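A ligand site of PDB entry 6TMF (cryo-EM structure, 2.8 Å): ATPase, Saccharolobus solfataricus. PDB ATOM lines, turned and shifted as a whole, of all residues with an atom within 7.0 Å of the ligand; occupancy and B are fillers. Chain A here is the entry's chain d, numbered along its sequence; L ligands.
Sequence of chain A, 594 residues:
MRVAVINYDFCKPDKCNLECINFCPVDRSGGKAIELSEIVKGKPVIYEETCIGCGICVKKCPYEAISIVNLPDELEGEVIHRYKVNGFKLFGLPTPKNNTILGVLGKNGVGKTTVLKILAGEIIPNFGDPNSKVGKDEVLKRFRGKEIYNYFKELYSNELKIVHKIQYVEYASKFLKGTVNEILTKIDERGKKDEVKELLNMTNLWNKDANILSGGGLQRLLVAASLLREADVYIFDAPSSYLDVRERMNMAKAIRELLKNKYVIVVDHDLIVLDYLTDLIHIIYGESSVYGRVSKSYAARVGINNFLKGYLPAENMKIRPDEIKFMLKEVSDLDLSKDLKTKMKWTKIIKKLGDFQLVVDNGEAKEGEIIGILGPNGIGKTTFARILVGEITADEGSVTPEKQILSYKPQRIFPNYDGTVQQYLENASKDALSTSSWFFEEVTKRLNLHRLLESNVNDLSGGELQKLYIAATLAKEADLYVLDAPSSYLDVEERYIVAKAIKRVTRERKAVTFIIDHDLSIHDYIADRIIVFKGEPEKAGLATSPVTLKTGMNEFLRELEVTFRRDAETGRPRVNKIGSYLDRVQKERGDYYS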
ATOM      1  N   ILE A   6      12.792  30.174  12.192  1.00  0.00           N
ATOM      2  CA  ILE A   6      12.911  29.917  13.611  1.00  0.00           C
ATOM      3  C   ILE A   6      11.570  30.105  14.275  1.00  0.00           C
ATOM      4  O   ILE A   6      10.766  30.947  13.864  1.00  0.00           O
ATOM      5  CB  ILE A   6      13.982  30.819  14.232  1.00  0.00           C
ATOM      6  CG1 ILE A   6      15.317  30.479  13.649  1.00  0.00           C
ATOM      7  CG2 ILE A   6      14.055  30.587  15.665  1.00  0.00           C
ATOM      8  CD1 ILE A   6      16.332  31.480  13.837  1.00  0.00           C
ATOM      9  N   ASN A   7      11.313  29.296  15.291  1.00  0.00           N
ATOM     10  CA  ASN A   7      10.052  29.339  16.004  1.00  0.00           C
ATOM     11  C   ASN A   7      10.055  30.413  17.072  1.00  0.00           C
ATOM     12  O   ASN A   7       9.006  31.006  17.331  1.00  0.00           O
ATOM     13  CB  ASN A   7       9.793  27.993  16.659  1.00  0.00           C
ATOM     14  CG  ASN A   7       8.361  27.822  17.057  1.00  0.00           C
ATOM     15  OD1 ASN A   7       7.544  28.716  16.888  1.00  0.00           O
ATOM     16  ND2 ASN A   7       8.053  26.656  17.596  1.00  0.00           N
ATOM     17  N   PHE A  10      10.872  27.936  21.057  1.00  0.00           N
ATOM     18  CA  PHE A  10      11.798  26.898  21.457  1.00  0.00           C
ATOM     19  C   PHE A  10      13.234  27.375  21.499  1.00  0.00           C
ATOM     20  O   PHE A  10      14.101  26.634  21.983  1.00  0.00           O
ATOM     21  CB  PHE A  10      11.700  25.715  20.504  1.00  0.00           C
ATOM     22  CG  PHE A  10      10.350  25.098  20.401  1.00  0.00           C
ATOM     23  CD1 PHE A  10       9.352  25.353  21.319  1.00  0.00           C
ATOM     24  CD2 PHE A  10      10.084  24.226  19.385  1.00  0.00           C
ATOM     25  CE1 PHE A  10       8.129  24.753  21.190  1.00  0.00           C
ATOM     26  CE2 PHE A  10       8.873  23.630  19.268  1.00  0.00           C
ATOM     27  CZ  PHE A  10       7.900  23.899  20.172  1.00  0.00           C
ATOM     28  N   CYS A  11      13.505  28.571  21.016  1.00  0.00           N
ATOM     29  CA  CYS A  11      14.872  29.054  20.940  1.00  0.00           C
ATOM     30  C   CYS A  11      15.329  29.551  22.288  1.00  0.00           C
ATOM     31  O   CYS A  11      14.638  30.326  22.960  1.00  0.00           O
ATOM     32  CB  CYS A  11      14.973  30.164  19.904  1.00  0.00           C
ATOM     33  SG  CYS A  11      16.414  31.174  20.025  1.00  0.00           S
ATOM     34  N   LYS A  12      16.510  29.118  22.690  1.00  0.00           N
ATOM     35  CA  LYS A  12      17.077  29.395  23.994  1.00  0.00           C
ATOM     36  C   LYS A  12      18.545  29.700  23.779  1.00  0.00           C
ATOM     37  O   LYS A  12      19.415  28.837  23.978  1.00  0.00           O
ATOM     38  CB  LYS A  12      16.866  28.228  24.934  1.00  0.00           C
ATOM     39  CG  LYS A  12      15.422  27.831  25.102  1.00  0.00           C
ATOM     40  CD  LYS A  12      15.280  26.583  25.928  1.00  0.00           C
ATOM     41  CE  LYS A  12      14.003  25.844  25.620  1.00  0.00           C
ATOM     42  NZ  LYS A  12      13.916  24.563  26.366  1.00  0.00           N
ATOM     43  N   PRO A  13      18.872  30.922  23.391  1.00  0.00           N
ATOM     44  CA  PRO A  13      20.250  31.241  23.018  1.00  0.00           C
ATOM     45  C   PRO A  13      21.293  31.057  24.110  1.00  0.00           C
ATOM     46  O   PRO A  13      22.491  31.165  23.871  1.00  0.00           O
ATOM     47  CB  PRO A  13      20.152  32.715  22.629  1.00  0.00           C
ATOM     48  CG  PRO A  13      18.791  32.912  22.284  1.00  0.00           C
ATOM     49  CD  PRO A  13      17.993  32.067  23.145  1.00  0.00           C
ATOM     50  N   ASP A  14      20.822  30.830  25.327  1.00  0.00           N
ATOM     51  CA  ASP A  14      21.677  30.694  26.486  1.00  0.00           C
ATOM     52  C   ASP A  14      22.165  29.271  26.638  1.00  0.00           C
ATOM     53  O   ASP A  14      23.355  29.015  26.855  1.00  0.00           O
ATOM     54  CB  ASP A  14      20.895  31.146  27.713  1.00  0.00           C
ATOM     55  CG  ASP A  14      20.089  32.389  27.436  1.00  0.00           C
ATOM     56  OD1 ASP A  14      20.614  33.284  26.738  1.00  0.00           O
ATOM     57  OD2 ASP A  14      18.931  32.463  27.881  1.00  0.00           O
ATOM     58  N   LYS A  15      21.242  28.329  26.556  1.00  0.00           N
ATOM     59  CA  LYS A  15      21.523  26.913  26.790  1.00  0.00           C
ATOM     60  C   LYS A  15      21.741  26.166  25.475  1.00  0.00           C
ATOM     61  O   LYS A  15      21.271  25.042  25.317  1.00  0.00           O
ATOM     62  CB  LYS A  15      20.359  26.302  27.554  1.00  0.00           C
ATOM     63  CG  LYS A  15      19.882  27.062  28.758  1.00  0.00           C
ATOM     64  CD  LYS A  15      18.465  26.689  29.129  1.00  0.00           C
ATOM     65  CE  LYS A  15      18.334  25.238  29.610  1.00  0.00           C
ATOM     66  NZ  LYS A  15      19.020  24.990  30.928  1.00  0.00           N
ATOM     67  N   CYS A  16      22.498  26.747  24.545  1.00  0.00           N
ATOM     68  CA  CYS A  16      22.571  26.230  23.185  1.00  0.00           C
ATOM     69  C   CYS A  16      23.970  26.106  22.619  1.00  0.00           C
ATOM     70  O   CYS A  16      24.183  25.231  21.766  1.00  0.00           O
ATOM     71  CB  CYS A  16      21.768  27.123  22.248  1.00  0.00           C
ATOM     72  SG  CYS A  16      22.514  28.690  21.970  1.00  0.00           S
ATOM     73  N   ASN A  17      24.908  26.942  23.033  1.00  0.00           N
ATOM     74  CA  ASN A  17      26.213  27.111  22.385  1.00  0.00           C
ATOM     75  C   ASN A  17      26.110  27.606  20.941  1.00  0.00           C
ATOM     76  O   ASN A  17      27.118  27.649  20.231  1.00  0.00           O
ATOM     77  CB  ASN A  17      27.027  25.816  22.448  1.00  0.00           C
ATOM     78  CG  ASN A  17      27.792  25.691  23.739  1.00  0.00           C
ATOM     79  OD1 ASN A  17      28.436  26.632  24.191  1.00  0.00           O
ATOM     80  ND2 ASN A  17      27.700  24.520  24.345  1.00  0.00           N
ATOM     81  N   LEU A  18      24.926  28.014  20.491  1.00  0.00           N
ATOM     82  CA  LEU A  18      24.729  28.682  19.207  1.00  0.00           C
ATOM     83  C   LEU A  18      25.218  27.824  18.039  1.00  0.00           C
ATOM     84  O   LEU A  18      25.904  28.276  17.113  1.00  0.00           O
ATOM     85  CB  LEU A  18      25.390  30.049  19.225  1.00  0.00           C
ATOM     86  CG  LEU A  18      24.556  31.065  19.959  1.00  0.00           C
ATOM     87  CD1 LEU A  18      24.849  31.091  21.405  1.00  0.00           C
ATOM     88  CD2 LEU A  18      24.785  32.400  19.405  1.00  0.00           C
ATOM     89  N   GLU A  19      24.778  26.578  18.068  1.00  0.00           N
ATOM     90  CA  GLU A  19      25.236  25.603  17.105  1.00  0.00           C
ATOM     91  C   GLU A  19      24.826  25.981  15.708  1.00  0.00           C
ATOM     92  O   GLU A  19      25.495  25.613  14.741  1.00  0.00           O
ATOM     93  CB  GLU A  19      24.685  24.238  17.456  1.00  0.00           C
ATOM     94  CG  GLU A  19      24.814  23.875  18.891  1.00  0.00           C
ATOM     95  CD  GLU A  19      24.612  22.403  19.164  1.00  0.00           C
ATOM     96  OE1 GLU A  19      24.853  21.578  18.257  1.00  0.00           O
ATOM     97  OE2 GLU A  19      24.194  22.061  20.288  1.00  0.00           O
ATOM     98  N   CYS A  20      23.744  26.738  15.568  1.00  0.00           N
ATOM     99  CA  CYS A  20      23.255  27.128  14.257  1.00  0.00           C
ATOM    100  C   CYS A  20      24.275  28.001  13.531  1.00  0.00           C
ATOM    101  O   CYS A  20      24.801  27.620  12.477  1.00  0.00           O
ATOM    102  CB  CYS A  20      21.935  27.842  14.433  1.00  0.00           C
ATOM    103  SG  CYS A  20      22.005  29.416  15.289  1.00  0.00           S
ATOM    104  N   ILE A  21      24.552  29.178  14.082  1.00  0.00           N
ATOM    105  CA  ILE A  21      25.532  30.061  13.478  1.00  0.00           C
ATOM    106  C   ILE A  21      26.863  29.351  13.358  1.00  0.00           C
ATOM    107  O   ILE A  21      27.583  29.539  12.371  1.00  0.00           O
ATOM    108  CB  ILE A  21      25.679  31.366  14.265  1.00  0.00           C
ATOM    109  CG1 ILE A  21      26.146  31.108  15.683  1.00  0.00           C
ATOM    110  CG2 ILE A  21      24.385  32.090  14.327  1.00  0.00           C
ATOM    111  CD1 ILE A  21      26.482  32.323  16.407  1.00  0.00           C
ATOM    112  N   ILE A  34      22.597  33.592   9.116  1.00  0.00           N
ATOM    113  CA  ILE A  34      22.070  33.575  10.469  1.00  0.00           C
ATOM    114  C   ILE A  34      22.891  34.515  11.300  1.00  0.00           C
ATOM    115  O   ILE A  34      24.125  34.501  11.233  1.00  0.00           O
ATOM    116  CB  ILE A  34      22.117  32.188  11.120  1.00  0.00           C
ATOM    117  CG1 ILE A  34      21.528  31.124  10.235  1.00  0.00           C
ATOM    118  CG2 ILE A  34      21.296  32.181  12.347  1.00  0.00           C
ATOM    119  CD1 ILE A  34      22.079  29.833  10.499  1.00  0.00           C
ATOM    120  N   LEU A  36      22.788  36.854  15.268  1.00  0.00           N
ATOM    121  CA  LEU A  36      22.120  37.356  16.446  1.00  0.00           C
ATOM    122  C   LEU A  36      21.564  38.749  16.188  1.00  0.00           C
ATOM    123  O   LEU A  36      21.976  39.427  15.242  1.00  0.00           O
ATOM    124  CB  LEU A  36      23.097  37.400  17.608  1.00  0.00           C
ATOM    125  CG  LEU A  36      23.606  36.023  18.011  1.00  0.00           C
ATOM    126  CD1 LEU A  36      24.802  36.143  18.907  1.00  0.00           C
ATOM    127  CD2 LEU A  36      22.522  35.270  18.687  1.00  0.00           C
ATOM    128  N   GLY A  42      17.780  39.011  21.822  1.00  0.00           N
ATOM    129  CA  GLY A  42      19.103  38.485  21.598  1.00  0.00           C
ATOM    130  C   GLY A  42      19.127  37.176  20.858  1.00  0.00           C
ATOM    131  O   GLY A  42      20.074  36.404  20.990  1.00  0.00           O
ATOM    132  N   LYS A  43      18.140  36.914  20.124  1.00  0.00           N
ATOM    133  CA  LYS A  43      17.880  35.677  19.431  1.00  0.00           C
ATOM    134  C   LYS A  43      18.270  35.806  17.971  1.00  0.00           C
ATOM    135  O   LYS A  43      18.350  36.918  17.430  1.00  0.00           O
ATOM    136  CB  LYS A  43      16.415  35.309  19.536  1.00  0.00           C
ATOM    137  CG  LYS A  43      16.011  34.783  20.899  1.00  0.00           C
ATOM    138  CD  LYS A  43      14.640  34.156  20.881  1.00  0.00           C
ATOM    139  CE  LYS A  43      14.375  33.303  22.097  1.00  0.00           C
ATOM    140  NZ  LYS A  43      13.513  33.978  23.079  1.00  0.00           N
ATOM    141  N   PRO A  44      18.511  34.691  17.301  1.00  0.00           N
ATOM    142  CA  PRO A  44      18.985  34.736  15.927  1.00  0.00           C
ATOM    143  C   PRO A  44      17.884  35.026  14.938  1.00  0.00           C
ATOM    144  O   PRO A  44      16.707  34.732  15.147  1.00  0.00           O
ATOM    145  CB  PRO A  44      19.538  33.337  15.724  1.00  0.00           C
ATOM    146  CG  PRO A  44      18.779  32.547  16.588  1.00  0.00           C
ATOM    147  CD  PRO A  44      18.567  33.313  17.806  1.00  0.00           C
ATOM    148  N   CYS A  57      21.551  23.851  10.376  1.00  0.00           N
ATOM    149  CA  CYS A  57      21.076  24.487  11.584  1.00  0.00           C
ATOM    150  C   CYS A  57      19.940  23.708  12.179  1.00  0.00           C
ATOM    151  O   CYS A  57      19.819  23.605  13.404  1.00  0.00           O
ATOM    152  CB  CYS A  57      20.624  25.904  11.246  1.00  0.00           C
ATOM    153  SG  CYS A  57      19.204  25.959  10.210  1.00  0.00           S
ATOM    154  N   LYS A  60      21.321  20.729  13.964  1.00  0.00           N
ATOM    155  CA  LYS A  60      22.262  21.066  15.018  1.00  0.00           C
ATOM    156  C   LYS A  60      21.617  21.699  16.215  1.00  0.00           C
ATOM    157  O   LYS A  60      22.064  21.481  17.344  1.00  0.00           O
ATOM    158  CB  LYS A  60      23.343  22.001  14.499  1.00  0.00           C
ATOM    159  CG  LYS A  60      24.350  21.384  13.628  1.00  0.00           C
ATOM    160  CD  LYS A  60      25.364  20.600  14.399  1.00  0.00           C
ATOM    161  CE  LYS A  60      25.948  19.504  13.583  1.00  0.00           C
ATOM    162  NZ  LYS A  60      24.950  18.469  13.330  1.00  0.00           N
ATOM    163  N   CYS A  61      20.591  22.506  16.008  1.00  0.00           N
ATOM    164  CA  CYS A  61      19.790  23.005  17.104  1.00  0.00           C
ATOM    165  C   CYS A  61      19.317  21.853  17.976  1.00  0.00           C
ATOM    166  O   CYS A  61      18.655  20.934  17.467  1.00  0.00           O
ATOM    167  CB  CYS A  61      18.585  23.749  16.575  1.00  0.00           C
ATOM    168  SG  CYS A  61      17.706  24.700  17.758  1.00  0.00           S
ATOM    169  N   PRO A  62      19.627  21.847  19.262  1.00  0.00           N
ATOM    170  CA  PRO A  62      19.164  20.770  20.126  1.00  0.00           C
ATOM    171  C   PRO A  62      17.675  20.820  20.376  1.00  0.00           C
ATOM    172  O   PRO A  62      16.999  19.788  20.401  1.00  0.00           O
ATOM    173  CB  PRO A  62      19.940  21.000  21.409  1.00  0.00           C
ATOM    174  CG  PRO A  62      20.949  21.976  21.095  1.00  0.00           C
ATOM    175  CD  PRO A  62      20.457  22.779  20.028  1.00  0.00           C
ATOM    176  N   TYR A  63      17.180  22.023  20.608  1.00  0.00           N
ATOM    177  CA  TYR A  63      15.755  22.269  20.762  1.00  0.00           C
ATOM    178  C   TYR A  63      15.213  22.560  19.377  1.00  0.00           C
ATOM    179  O   TYR A  63      15.299  23.690  18.891  1.00  0.00           O
ATOM    180  CB  TYR A  63      15.497  23.428  21.698  1.00  0.00           C
ATOM    181  CG  TYR A  63      16.413  23.485  22.885  1.00  0.00           C
ATOM    182  CD1 TYR A  63      17.242  24.553  23.073  1.00  0.00           C
ATOM    183  CD2 TYR A  63      16.446  22.465  23.815  1.00  0.00           C
ATOM    184  CE1 TYR A  63      18.076  24.620  24.137  1.00  0.00           C
ATOM    185  CE2 TYR A  63      17.275  22.516  24.881  1.00  0.00           C
ATOM    186  CZ  TYR A  63      18.094  23.602  25.048  1.00  0.00           C
ATOM    187  OH  TYR A  63      18.932  23.662  26.119  1.00  0.00           O
ATOM    188  N   GLU A  64      14.546  21.584  18.780  1.00  0.00           N
ATOM    189  CA  GLU A  64      14.357  21.564  17.336  1.00  0.00           C
ATOM    190  C   GLU A  64      13.462  22.743  16.960  1.00  0.00           C
ATOM    191  O   GLU A  64      12.266  22.622  16.701  1.00  0.00           O
ATOM    192  CB  GLU A  64      13.771  20.243  16.894  1.00  0.00           C
ATOM    193  CG  GLU A  64      14.575  19.057  17.332  1.00  0.00           C
ATOM    194  CD  GLU A  64      14.005  17.745  16.821  1.00  0.00           C
ATOM    195  OE1 GLU A  64      13.125  17.798  15.935  1.00  0.00           O
ATOM    196  OE2 GLU A  64      14.429  16.678  17.305  1.00  0.00           O
ATOM    197  N   ALA A  65      14.109  23.897  16.900  1.00  0.00           N
ATOM    198  CA  ALA A  65      13.507  25.194  16.747  1.00  0.00           C
ATOM    199  C   ALA A  65      13.505  25.688  15.326  1.00  0.00           C
ATOM    200  O   ALA A  65      12.665  26.516  14.973  1.00  0.00           O
ATOM    201  CB  ALA A  65      14.269  26.191  17.569  1.00  0.00           C
ATOM    202  N   ILE A  66      14.444  25.232  14.526  1.00  0.00           N
ATOM    203  CA  ILE A  66      14.585  25.664  13.156  1.00  0.00           C
ATOM    204  C   ILE A  66      13.919  24.638  12.253  1.00  0.00           C
ATOM    205  O   ILE A  66      13.989  23.436  12.499  1.00  0.00           O
ATOM    206  CB  ILE A  66      16.060  25.847  12.778  1.00  0.00           C
ATOM    207  CG1 ILE A  66      16.724  26.830  13.715  1.00  0.00           C
ATOM    208  CG2 ILE A  66      16.158  26.363  11.402  1.00  0.00           C
ATOM    209  CD1 ILE A  66      18.144  26.823  13.684  1.00  0.00           C
HETATM  210 FE1  LIG L   1      19.743  28.663  17.353  1.00  0.00          FE
HETATM  211 FE2  LIG L   1      20.355  28.047  19.942  1.00  0.00          FE
HETATM  212 FE3  LIG L   1      18.865  26.341  18.458  1.00  0.00          FE
HETATM  213 FE4  LIG L   1      17.803  28.708  19.280  1.00  0.00          FE
HETATM  214  S1  LIG L   1      18.462  26.979  20.592  1.00  0.00           S
HETATM  215  S2  LIG L   1      17.654  27.799  17.197  1.00  0.00           S
HETATM  216  S3  LIG L   1      19.642  30.049  19.149  1.00  0.00           S
HETATM  217  S4  LIG L   1      21.024  26.929  18.070  1.00  0.00           S
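N of Glu 19 sits close to S4 of the ligand, 3.8 Å away. SG of Cys 11 lies close to S3 of the ligand (3.5 Å). The backbone NH (N) of Lys 12 lies close to a sulfur (S1) of the ligand (3.6 Å). N of Cys 20 sits close to S4 of the ligand (3.7 Å). The side-chain sulfur (SG) of Cys 61 is bound to an iron atom (FE3) of the ligand, at 2.1 Å.
Merely in contact with the ligand: Cys 16, Pro 44, Tyr 63, Ala 65 and Ile 66. Of the 27 residues printed, 10 come within 4 Å of the ligand.
The side-chain sulfur of Cys 61 sits close to the backbone NH of Ala 65, at 3.8 Å. SG of Cys 16 is in hydrogen-bond range of O of Pro 13, 3.1 Å away. The side-chain sulfur of Cys 16 is in hydrogen-bond range of the backbone NH of Leu 18 (2.9 Å). The side-chain hydroxyl of Tyr 63 is in hydrogen-bond range of the backbone carbonyl oxygen of Lys 15 (2.8 Å). O of Lys 12 lies close to SG of Cys 16 (3.7 Å). The backbone NH (N) of Asn 7 lies within hydrogen-bond range of the backbone carbonyl oxygen (O) of Ala 65 (3.1 Å). The side-chain sulfur (SG) of Cys 61 lies close to the backbone carbonyl oxygen (O) of Tyr 63, 2.8 Å away.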
